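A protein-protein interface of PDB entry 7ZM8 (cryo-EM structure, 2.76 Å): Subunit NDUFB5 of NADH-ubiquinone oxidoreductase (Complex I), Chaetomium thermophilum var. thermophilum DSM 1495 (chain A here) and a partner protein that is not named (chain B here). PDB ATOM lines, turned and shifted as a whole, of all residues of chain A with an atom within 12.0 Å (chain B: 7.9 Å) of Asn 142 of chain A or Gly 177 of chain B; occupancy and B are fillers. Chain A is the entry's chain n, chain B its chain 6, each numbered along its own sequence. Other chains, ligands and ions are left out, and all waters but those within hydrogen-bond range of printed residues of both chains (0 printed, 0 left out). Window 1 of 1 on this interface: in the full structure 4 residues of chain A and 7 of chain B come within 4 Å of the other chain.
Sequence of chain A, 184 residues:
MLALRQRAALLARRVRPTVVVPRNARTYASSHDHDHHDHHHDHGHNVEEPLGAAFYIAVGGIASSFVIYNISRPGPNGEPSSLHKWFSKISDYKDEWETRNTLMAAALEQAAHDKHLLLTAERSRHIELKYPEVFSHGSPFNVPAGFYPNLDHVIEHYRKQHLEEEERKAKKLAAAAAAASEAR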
ATOM      1  N   GLY A 138      28.412 -12.229  -1.421  1.00  0.00           N
ATOM      2  CA  GLY A 138      27.175 -12.700  -2.065  1.00  0.00           C
ATOM      3  C   GLY A 138      26.414 -11.591  -2.764  1.00  0.00           C
ATOM      4  O   GLY A 138      26.282 -10.531  -2.167  1.00  0.00           O
ATOM      5  N   SER A 139      25.882 -11.837  -3.961  1.00  0.00           N
ATOM      6  CA  SER A 139      25.077 -10.806  -4.592  1.00  0.00           C
ATOM      7  C   SER A 139      23.806 -10.554  -3.788  1.00  0.00           C
ATOM      8  O   SER A 139      23.153 -11.499  -3.338  1.00  0.00           O
ATOM      9  CB  SER A 139      24.717 -11.211  -6.019  1.00  0.00           C
ATOM     10  OG  SER A 139      23.892 -10.241  -6.635  1.00  0.00           O
ATOM     11  N   PRO A 140      23.431  -9.293  -3.586  1.00  0.00           N
ATOM     12  CA  PRO A 140      22.158  -8.969  -2.933  1.00  0.00           C
ATOM     13  C   PRO A 140      20.975  -8.814  -3.877  1.00  0.00           C
ATOM     14  O   PRO A 140      19.923  -8.348  -3.437  1.00  0.00           O
ATOM     15  CB  PRO A 140      22.484  -7.632  -2.263  1.00  0.00           C
ATOM     16  CG  PRO A 140      23.448  -6.998  -3.189  1.00  0.00           C
ATOM     17  CD  PRO A 140      24.225  -8.086  -3.868  1.00  0.00           C
ATOM     18  N   PHE A 141      21.124  -9.202  -5.140  1.00  0.00           N
ATOM     19  CA  PHE A 141      20.049  -8.995  -6.141  1.00  0.00           C
ATOM     20  C   PHE A 141      19.576 -10.332  -6.687  1.00  0.00           C
ATOM     21  O   PHE A 141      20.407 -11.239  -6.783  1.00  0.00           O
ATOM     22  CB  PHE A 141      20.559  -8.174  -7.323  1.00  0.00           C
ATOM     23  CG  PHE A 141      21.403  -6.985  -6.944  1.00  0.00           C
ATOM     24  CD1 PHE A 141      20.855  -5.922  -6.246  1.00  0.00           C
ATOM     25  CD2 PHE A 141      22.742  -6.929  -7.290  1.00  0.00           C
ATOM     26  CE1 PHE A 141      21.631  -4.832  -5.895  1.00  0.00           C
ATOM     27  CE2 PHE A 141      23.517  -5.838  -6.940  1.00  0.00           C
ATOM     28  CZ  PHE A 141      22.960  -4.794  -6.241  1.00  0.00           C
ATOM     29  N   ASN A 142      18.282 -10.441  -6.992  1.00  0.00           N
ATOM     30  CA  ASN A 142      17.732 -11.659  -7.641  1.00  0.00           C
ATOM     31  C   ASN A 142      18.037 -12.843  -6.742  1.00  0.00           C
ATOM     32  O   ASN A 142      18.335 -13.922  -7.264  1.00  0.00           O
ATOM     33  CB  ASN A 142      18.200 -11.777  -9.094  1.00  0.00           C
ATOM     34  CG  ASN A 142      17.899 -10.544  -9.911  1.00  0.00           C
ATOM     35  OD1 ASN A 142      16.797 -10.009  -9.843  1.00  0.00           O
ATOM     36  ND2 ASN A 142      18.874 -10.087 -10.676  1.00  0.00           N
ATOM     37  N   VAL A 143      17.951 -12.618  -5.438  1.00  0.00           N
ATOM     38  CA  VAL A 143      18.271 -13.683  -4.453  1.00  0.00           C
ATOM     39  C   VAL A 143      17.043 -14.579  -4.295  1.00  0.00           C
ATOM     40  O   VAL A 143      15.986 -14.033  -3.938  1.00  0.00           O
ATOM     41  CB  VAL A 143      18.723 -13.083  -3.111  1.00  0.00           C
ATOM     42  CG1 VAL A 143      18.898 -14.154  -2.048  1.00  0.00           C
ATOM     43  CG2 VAL A 143      19.984 -12.257  -3.261  1.00  0.00           C
ATOM     44  N   PRO A 144      17.088 -15.908  -4.577  1.00  0.00           N
ATOM     45  CA  PRO A 144      15.915 -16.718  -4.304  1.00  0.00           C
ATOM     46  C   PRO A 144      15.758 -17.084  -2.824  1.00  0.00           C
ATOM     47  O   PRO A 144      16.743 -17.229  -2.165  1.00  0.00           O
ATOM     48  CB  PRO A 144      16.271 -18.008  -5.038  1.00  0.00           C
ATOM     49  CG  PRO A 144      17.466 -17.690  -5.909  1.00  0.00           C
ATOM     50  CD  PRO A 144      18.216 -16.629  -5.146  1.00  0.00           C
ATOM     51  N   ALA A 145      14.536 -17.136  -2.307  1.00  0.00           N
ATOM     52  CA  ALA A 145      14.288 -17.463  -0.883  1.00  0.00           C
ATOM     53  C   ALA A 145      14.913 -18.813  -0.520  1.00  0.00           C
ATOM     54  O   ALA A 145      14.737 -19.780  -1.289  1.00  0.00           O
ATOM     55  CB  ALA A 145      12.821 -17.425  -0.573  1.00  0.00           C
ATOM     56  N   GLY A 146      15.614 -18.869   0.607  1.00  0.00           N
ATOM     57  CA  GLY A 146      16.245 -20.117   1.050  1.00  0.00           C
ATOM     58  C   GLY A 146      17.543 -20.393   0.337  1.00  0.00           C
ATOM     59  O   GLY A 146      18.090 -21.491   0.530  1.00  0.00           O
ATOM     60  N   PHE A 147      18.012 -19.473  -0.498  1.00  0.00           N
ATOM     61  CA  PHE A 147      19.330 -19.673  -1.142  1.00  0.00           C
ATOM     62  C   PHE A 147      20.457 -19.559  -0.125  1.00  0.00           C
ATOM     63  O   PHE A 147      21.269 -20.482  -0.044  1.00  0.00           O
ATOM     64  CB  PHE A 147      19.514 -18.696  -2.306  1.00  0.00           C
ATOM     65  CG  PHE A 147      20.869 -18.720  -2.956  1.00  0.00           C
ATOM     66  CD1 PHE A 147      21.914 -17.974  -2.440  1.00  0.00           C
ATOM     67  CD2 PHE A 147      21.090 -19.479  -4.090  1.00  0.00           C
ATOM     68  CE1 PHE A 147      23.161 -18.005  -3.032  1.00  0.00           C
ATOM     69  CE2 PHE A 147      22.335 -19.493  -4.693  1.00  0.00           C
ATOM     70  CZ  PHE A 147      23.361 -18.752  -4.162  1.00  0.00           C
ATOM     71  N   TYR A 148      20.462 -18.502   0.675  1.00  0.00           N
ATOM     72  CA  TYR A 148      21.620 -18.273   1.573  1.00  0.00           C
ATOM     73  C   TYR A 148      21.497 -19.070   2.862  1.00  0.00           C
ATOM     74  O   TYR A 148      20.450 -19.032   3.500  1.00  0.00           O
ATOM     75  CB  TYR A 148      21.821 -16.799   1.887  1.00  0.00           C
ATOM     76  CG  TYR A 148      22.473 -15.985   0.805  1.00  0.00           C
ATOM     77  CD1 TYR A 148      23.834 -16.060   0.577  1.00  0.00           C
ATOM     78  CD2 TYR A 148      21.728 -15.115   0.031  1.00  0.00           C
ATOM     79  CE1 TYR A 148      24.436 -15.296  -0.405  1.00  0.00           C
ATOM     80  CE2 TYR A 148      22.314 -14.349  -0.958  1.00  0.00           C
ATOM     81  CZ  TYR A 148      23.672 -14.441  -1.175  1.00  0.00           C
ATOM     82  OH  TYR A 148      24.246 -13.701  -2.156  1.00  0.00           O
ATOM     83  N   LYS B 173      12.594 -23.248 -15.138  1.00  0.00           N
ATOM     84  CA  LYS B 173      12.441 -21.785 -14.931  1.00  0.00           C
ATOM     85  C   LYS B 173      12.402 -21.416 -13.444  1.00  0.00           C
ATOM     86  O   LYS B 173      12.007 -22.272 -12.651  1.00  0.00           O
ATOM     87  CB  LYS B 173      11.157 -21.371 -15.657  1.00  0.00           C
ATOM     88  CG  LYS B 173       9.840 -21.683 -14.971  1.00  0.00           C
ATOM     89  CD  LYS B 173       8.662 -21.038 -15.666  1.00  0.00           C
ATOM     90  CE  LYS B 173       8.752 -21.101 -17.177  1.00  0.00           C
ATOM     91  NZ  LYS B 173       7.458 -20.794 -17.833  1.00  0.00           N
ATOM     92  N   ILE B 174      12.798 -20.193 -13.076  1.00  0.00           N
ATOM     93  CA  ILE B 174      12.717 -19.694 -11.665  1.00  0.00           C
ATOM     94  C   ILE B 174      12.066 -18.314 -11.699  1.00  0.00           C
ATOM     95  O   ILE B 174      12.173 -17.656 -12.725  1.00  0.00           O
ATOM     96  CB  ILE B 174      14.099 -19.637 -10.972  1.00  0.00           C
ATOM     97  CG1 ILE B 174      13.993 -19.422  -9.463  1.00  0.00           C
ATOM     98  CG2 ILE B 174      15.011 -18.607 -11.617  1.00  0.00           C
ATOM     99  CD1 ILE B 174      15.328 -19.472  -8.767  1.00  0.00           C
ATOM    100  N   TRP B 175      11.454 -17.876 -10.601  1.00  0.00           N
ATOM    101  CA  TRP B 175      10.719 -16.586 -10.620  1.00  0.00           C
ATOM    102  C   TRP B 175      11.378 -15.559  -9.700  1.00  0.00           C
ATOM    103  O   TRP B 175      11.537 -14.406 -10.125  1.00  0.00           O
ATOM    104  CB  TRP B 175       9.246 -16.817 -10.288  1.00  0.00           C
ATOM    105  CG  TRP B 175       8.547 -17.579 -11.370  1.00  0.00           C
ATOM    106  CD1 TRP B 175       8.232 -18.906 -11.374  1.00  0.00           C
ATOM    107  CD2 TRP B 175       8.114 -17.061 -12.639  1.00  0.00           C
ATOM    108  NE1 TRP B 175       7.611 -19.243 -12.544  1.00  0.00           N
ATOM    109  CE2 TRP B 175       7.527 -18.133 -13.342  1.00  0.00           C
ATOM    110  CE3 TRP B 175       8.156 -15.800 -13.244  1.00  0.00           C
ATOM    111  CZ2 TRP B 175       6.983 -17.978 -14.615  1.00  0.00           C
ATOM    112  CZ3 TRP B 175       7.620 -15.648 -14.500  1.00  0.00           C
ATOM    113  CH2 TRP B 175       7.039 -16.723 -15.172  1.00  0.00           C
ATOM    114  N   ASP B 176      11.731 -15.963  -8.485  1.00  0.00           N
ATOM    115  CA  ASP B 176      12.397 -15.047  -7.522  1.00  0.00           C
ATOM    116  C   ASP B 176      13.764 -14.612  -8.067  1.00  0.00           C
ATOM    117  O   ASP B 176      14.131 -13.445  -7.845  1.00  0.00           O
ATOM    118  CB  ASP B 176      12.350 -15.579  -6.083  1.00  0.00           C
ATOM    119  CG  ASP B 176      12.662 -17.056  -5.916  1.00  0.00           C
ATOM    120  OD1 ASP B 176      13.203 -17.655  -6.860  1.00  0.00           O
ATOM    121  OD2 ASP B 176      12.365 -17.591  -4.833  1.00  0.00           O
ATOM    122  N   GLY B 177      14.488 -15.511  -8.733  1.00  0.00           N
ATOM    123  CA  GLY B 177      15.803 -15.181  -9.314  1.00  0.00           C
ATOM    124  C   GLY B 177      15.712 -14.558 -10.697  1.00  0.00           C
ATOM    125  O   GLY B 177      16.772 -14.334 -11.300  1.00  0.00           O
ATOM    126  N   ALA B 178      14.503 -14.297 -11.198  1.00  0.00           N
ATOM    127  CA  ALA B 178      14.309 -13.618 -12.497  1.00  0.00           C
ATOM    128  C   ALA B 178      13.725 -12.222 -12.323  1.00  0.00           C
ATOM    129  O   ALA B 178      13.420 -11.631 -13.360  1.00  0.00           O
ATOM    130  CB  ALA B 178      13.385 -14.451 -13.345  1.00  0.00           C
ATOM    131  N   LEU B 179      13.550 -11.710 -11.102  1.00  0.00           N
ATOM    132  CA  LEU B 179      12.842 -10.408 -10.903  1.00  0.00           C
ATOM    133  C   LEU B 179      13.455  -9.298 -11.752  1.00  0.00           C
ATOM    134  O   LEU B 179      12.710  -8.637 -12.462  1.00  0.00           O
ATOM    135  CB  LEU B 179      12.864 -10.016  -9.424  1.00  0.00           C
ATOM    136  CG  LEU B 179      12.327  -8.629  -9.074  1.00  0.00           C
ATOM    137  CD1 LEU B 179      10.819  -8.566  -9.240  1.00  0.00           C
ATOM    138  CD2 LEU B 179      12.709  -8.245  -7.654  1.00  0.00           C
ATOM    139  N   ALA B 180      14.768  -9.127 -11.684  1.00  0.00           N
ATOM    140  CA  ALA B 180      15.460  -8.056 -12.411  1.00  0.00           C
ATOM    141  C   ALA B 180      16.725  -8.637 -13.015  1.00  0.00           C
ATOM    142  O   ALA B 180      17.798  -8.211 -12.617  1.00  0.00           O
ATOM    143  CB  ALA B 180      15.798  -6.989 -11.419  1.00  0.00           C
ATOM    144  N   GLU B 181      16.608  -9.543 -13.969  1.00  0.00           N
ATOM    145  CA  GLU B 181      17.817 -10.210 -14.504  1.00  0.00           C
ATOM    146  C   GLU B 181      18.712  -9.190 -15.204  1.00  0.00           C
ATOM    147  O   GLU B 181      18.194  -8.298 -15.900  1.00  0.00           O
ATOM    148  CB  GLU B 181      17.468 -11.433 -15.354  1.00  0.00           C
ATOM    149  CG  GLU B 181      18.583 -11.940 -16.249  1.00  0.00           C
ATOM    150  CD  GLU B 181      18.490 -11.481 -17.696  1.00  0.00           C
ATOM    151  OE1 GLU B 181      17.453 -10.897 -18.060  1.00  0.00           O
ATOM    152  OE2 GLU B 181      19.456 -11.700 -18.451  1.00  0.00           O
ATOM    153  N   ASN B 182      20.022  -9.347 -15.037  1.00  0.00           N
ATOM    154  CA  ASN B 182      20.969  -8.383 -15.625  1.00  0.00           C
ATOM    155  C   ASN B 182      21.690  -9.050 -16.774  1.00  0.00           C
ATOM    156  O   ASN B 182      21.776 -10.280 -16.771  1.00  0.00           O
ATOM    157  CB  ASN B 182      22.030  -7.904 -14.633  1.00  0.00           C
ATOM    158  CG  ASN B 182      21.483  -7.200 -13.416  1.00  0.00           C
ATOM    159  OD1 ASN B 182      20.287  -6.959 -13.307  1.00  0.00           O
ATOM    160  ND2 ASN B 182      22.362  -6.870 -12.491  1.00  0.00           N
ATOM    161  N   SER B 187      26.117  -7.235 -14.741  1.00  0.00           N
ATOM    162  CA  SER B 187      26.613  -8.048 -13.608  1.00  0.00           C
ATOM    163  C   SER B 187      28.119  -7.845 -13.367  1.00  0.00           C
ATOM    164  O   SER B 187      28.504  -7.770 -12.196  1.00  0.00           O
ATOM    165  CB  SER B 187      26.254  -9.474 -13.864  1.00  0.00           C
ATOM    166  OG  SER B 187      24.951  -9.571 -14.401  1.00  0.00           O
ATOM    167  N   ASN B 190      28.417  -4.437 -11.858  1.00  0.00           N
ATOM    168  CA  ASN B 190      27.961  -4.377 -10.454  1.00  0.00           C
ATOM    169  C   ASN B 190      29.130  -4.668  -9.517  1.00  0.00           C
ATOM    170  O   ASN B 190      29.141  -4.097  -8.431  1.00  0.00           O
ATOM    171  CB  ASN B 190      26.823  -5.354 -10.170  1.00  0.00           C
ATOM    172  CG  ASN B 190      25.500  -5.014 -10.818  1.00  0.00           C
ATOM    173  OD1 ASN B 190      25.317  -3.930 -11.359  1.00  0.00           O
ATOM    174  ND2 ASN B 190      24.570  -5.949 -10.768  1.00  0.00           N
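Asn 190 of chain B touches Phe 141 of chain A (ND2 to CE2, 3.97 Å). Asn 142 of chain A touches Gly 177 of chain B. N of Leu 179 of chain B touches OD1 of Asn 142 of chain A (3.9 Å). Asn 142 of chain A touches Glu 181 of chain B. Pro 144 of chain A touches Ile 174 of chain B. Asp 176 of chain B touches Pro 144 of chain A (OD1 to CB, 3.6 Å).
The backbone NH of Phe 141 of chain A lies close to the side-chain hydroxyl of Ser 139 of chain A (3.3 Å). O of Ala 180 of chain B lies close to OD1 of Asn 182 of chain B, 2.9 Å away. ND2 of Asn 182 of chain B sits close to ND2 of Asn 190 of chain B.
Hydrophobic or aromatic side chains of chain A that line the printed part of chain B: Phe 141 and Pro 144. Of the 12 printed residues of chain B, 7 touch a printed residue of chain A. Printed residues of chain B that touch a printed residue of chain A: Ile 174, Asp 176, Gly 177, Leu 179, Ala 180, Glu 181 and Asn 190. Among the printed residues, no Asp or Glu carboxylate lies within 4 Å of a Lys or Arg side-chain nitrogen of the other chain.
Printed residues of chain B within 4 Å of Phe 141 of chain A: Asn 190 (3.97 Å). Of chain B, only Gly 177 (3.5 Å), Leu 179 (3.9 Å), Ala 180 (2.9 Å) and Glu 181 (3.97 Å) come within 4 Å of Asn 142 of chain A. Of chain A, only Asn 142 comes within 4 Å of Gly 177 of chain B. No residue of chain A comes within 4 Å of Ala 178 of chain B. Of chain A, only Asn 142 (2.9 Å) comes within 4 Å of Ala 180 of chain B. Of the printed residues of chain A, Glu 181 of chain B touches Asn 142. No residue of chain A comes within 4 Å of Asn 182 of chain B. Of the printed residues of chain A, Asn 190 of chain B touches Phe 141. The nearest residue of chain A that does not touch Gly 177 of chain B is Pro 144 of chain A (4.5 Å).
The side-chain amide oxygen of Asn 142 of chain A lies within hydrogen-bond range of the backbone NH of Ala 180 of chain B (2.9 Å). The side-chain carboxylate (OD2) of Asp 176 of chain B lies within hydrogen-bond range of the backbone NH (N) of Ala 145 of chain A (3.4 Å).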
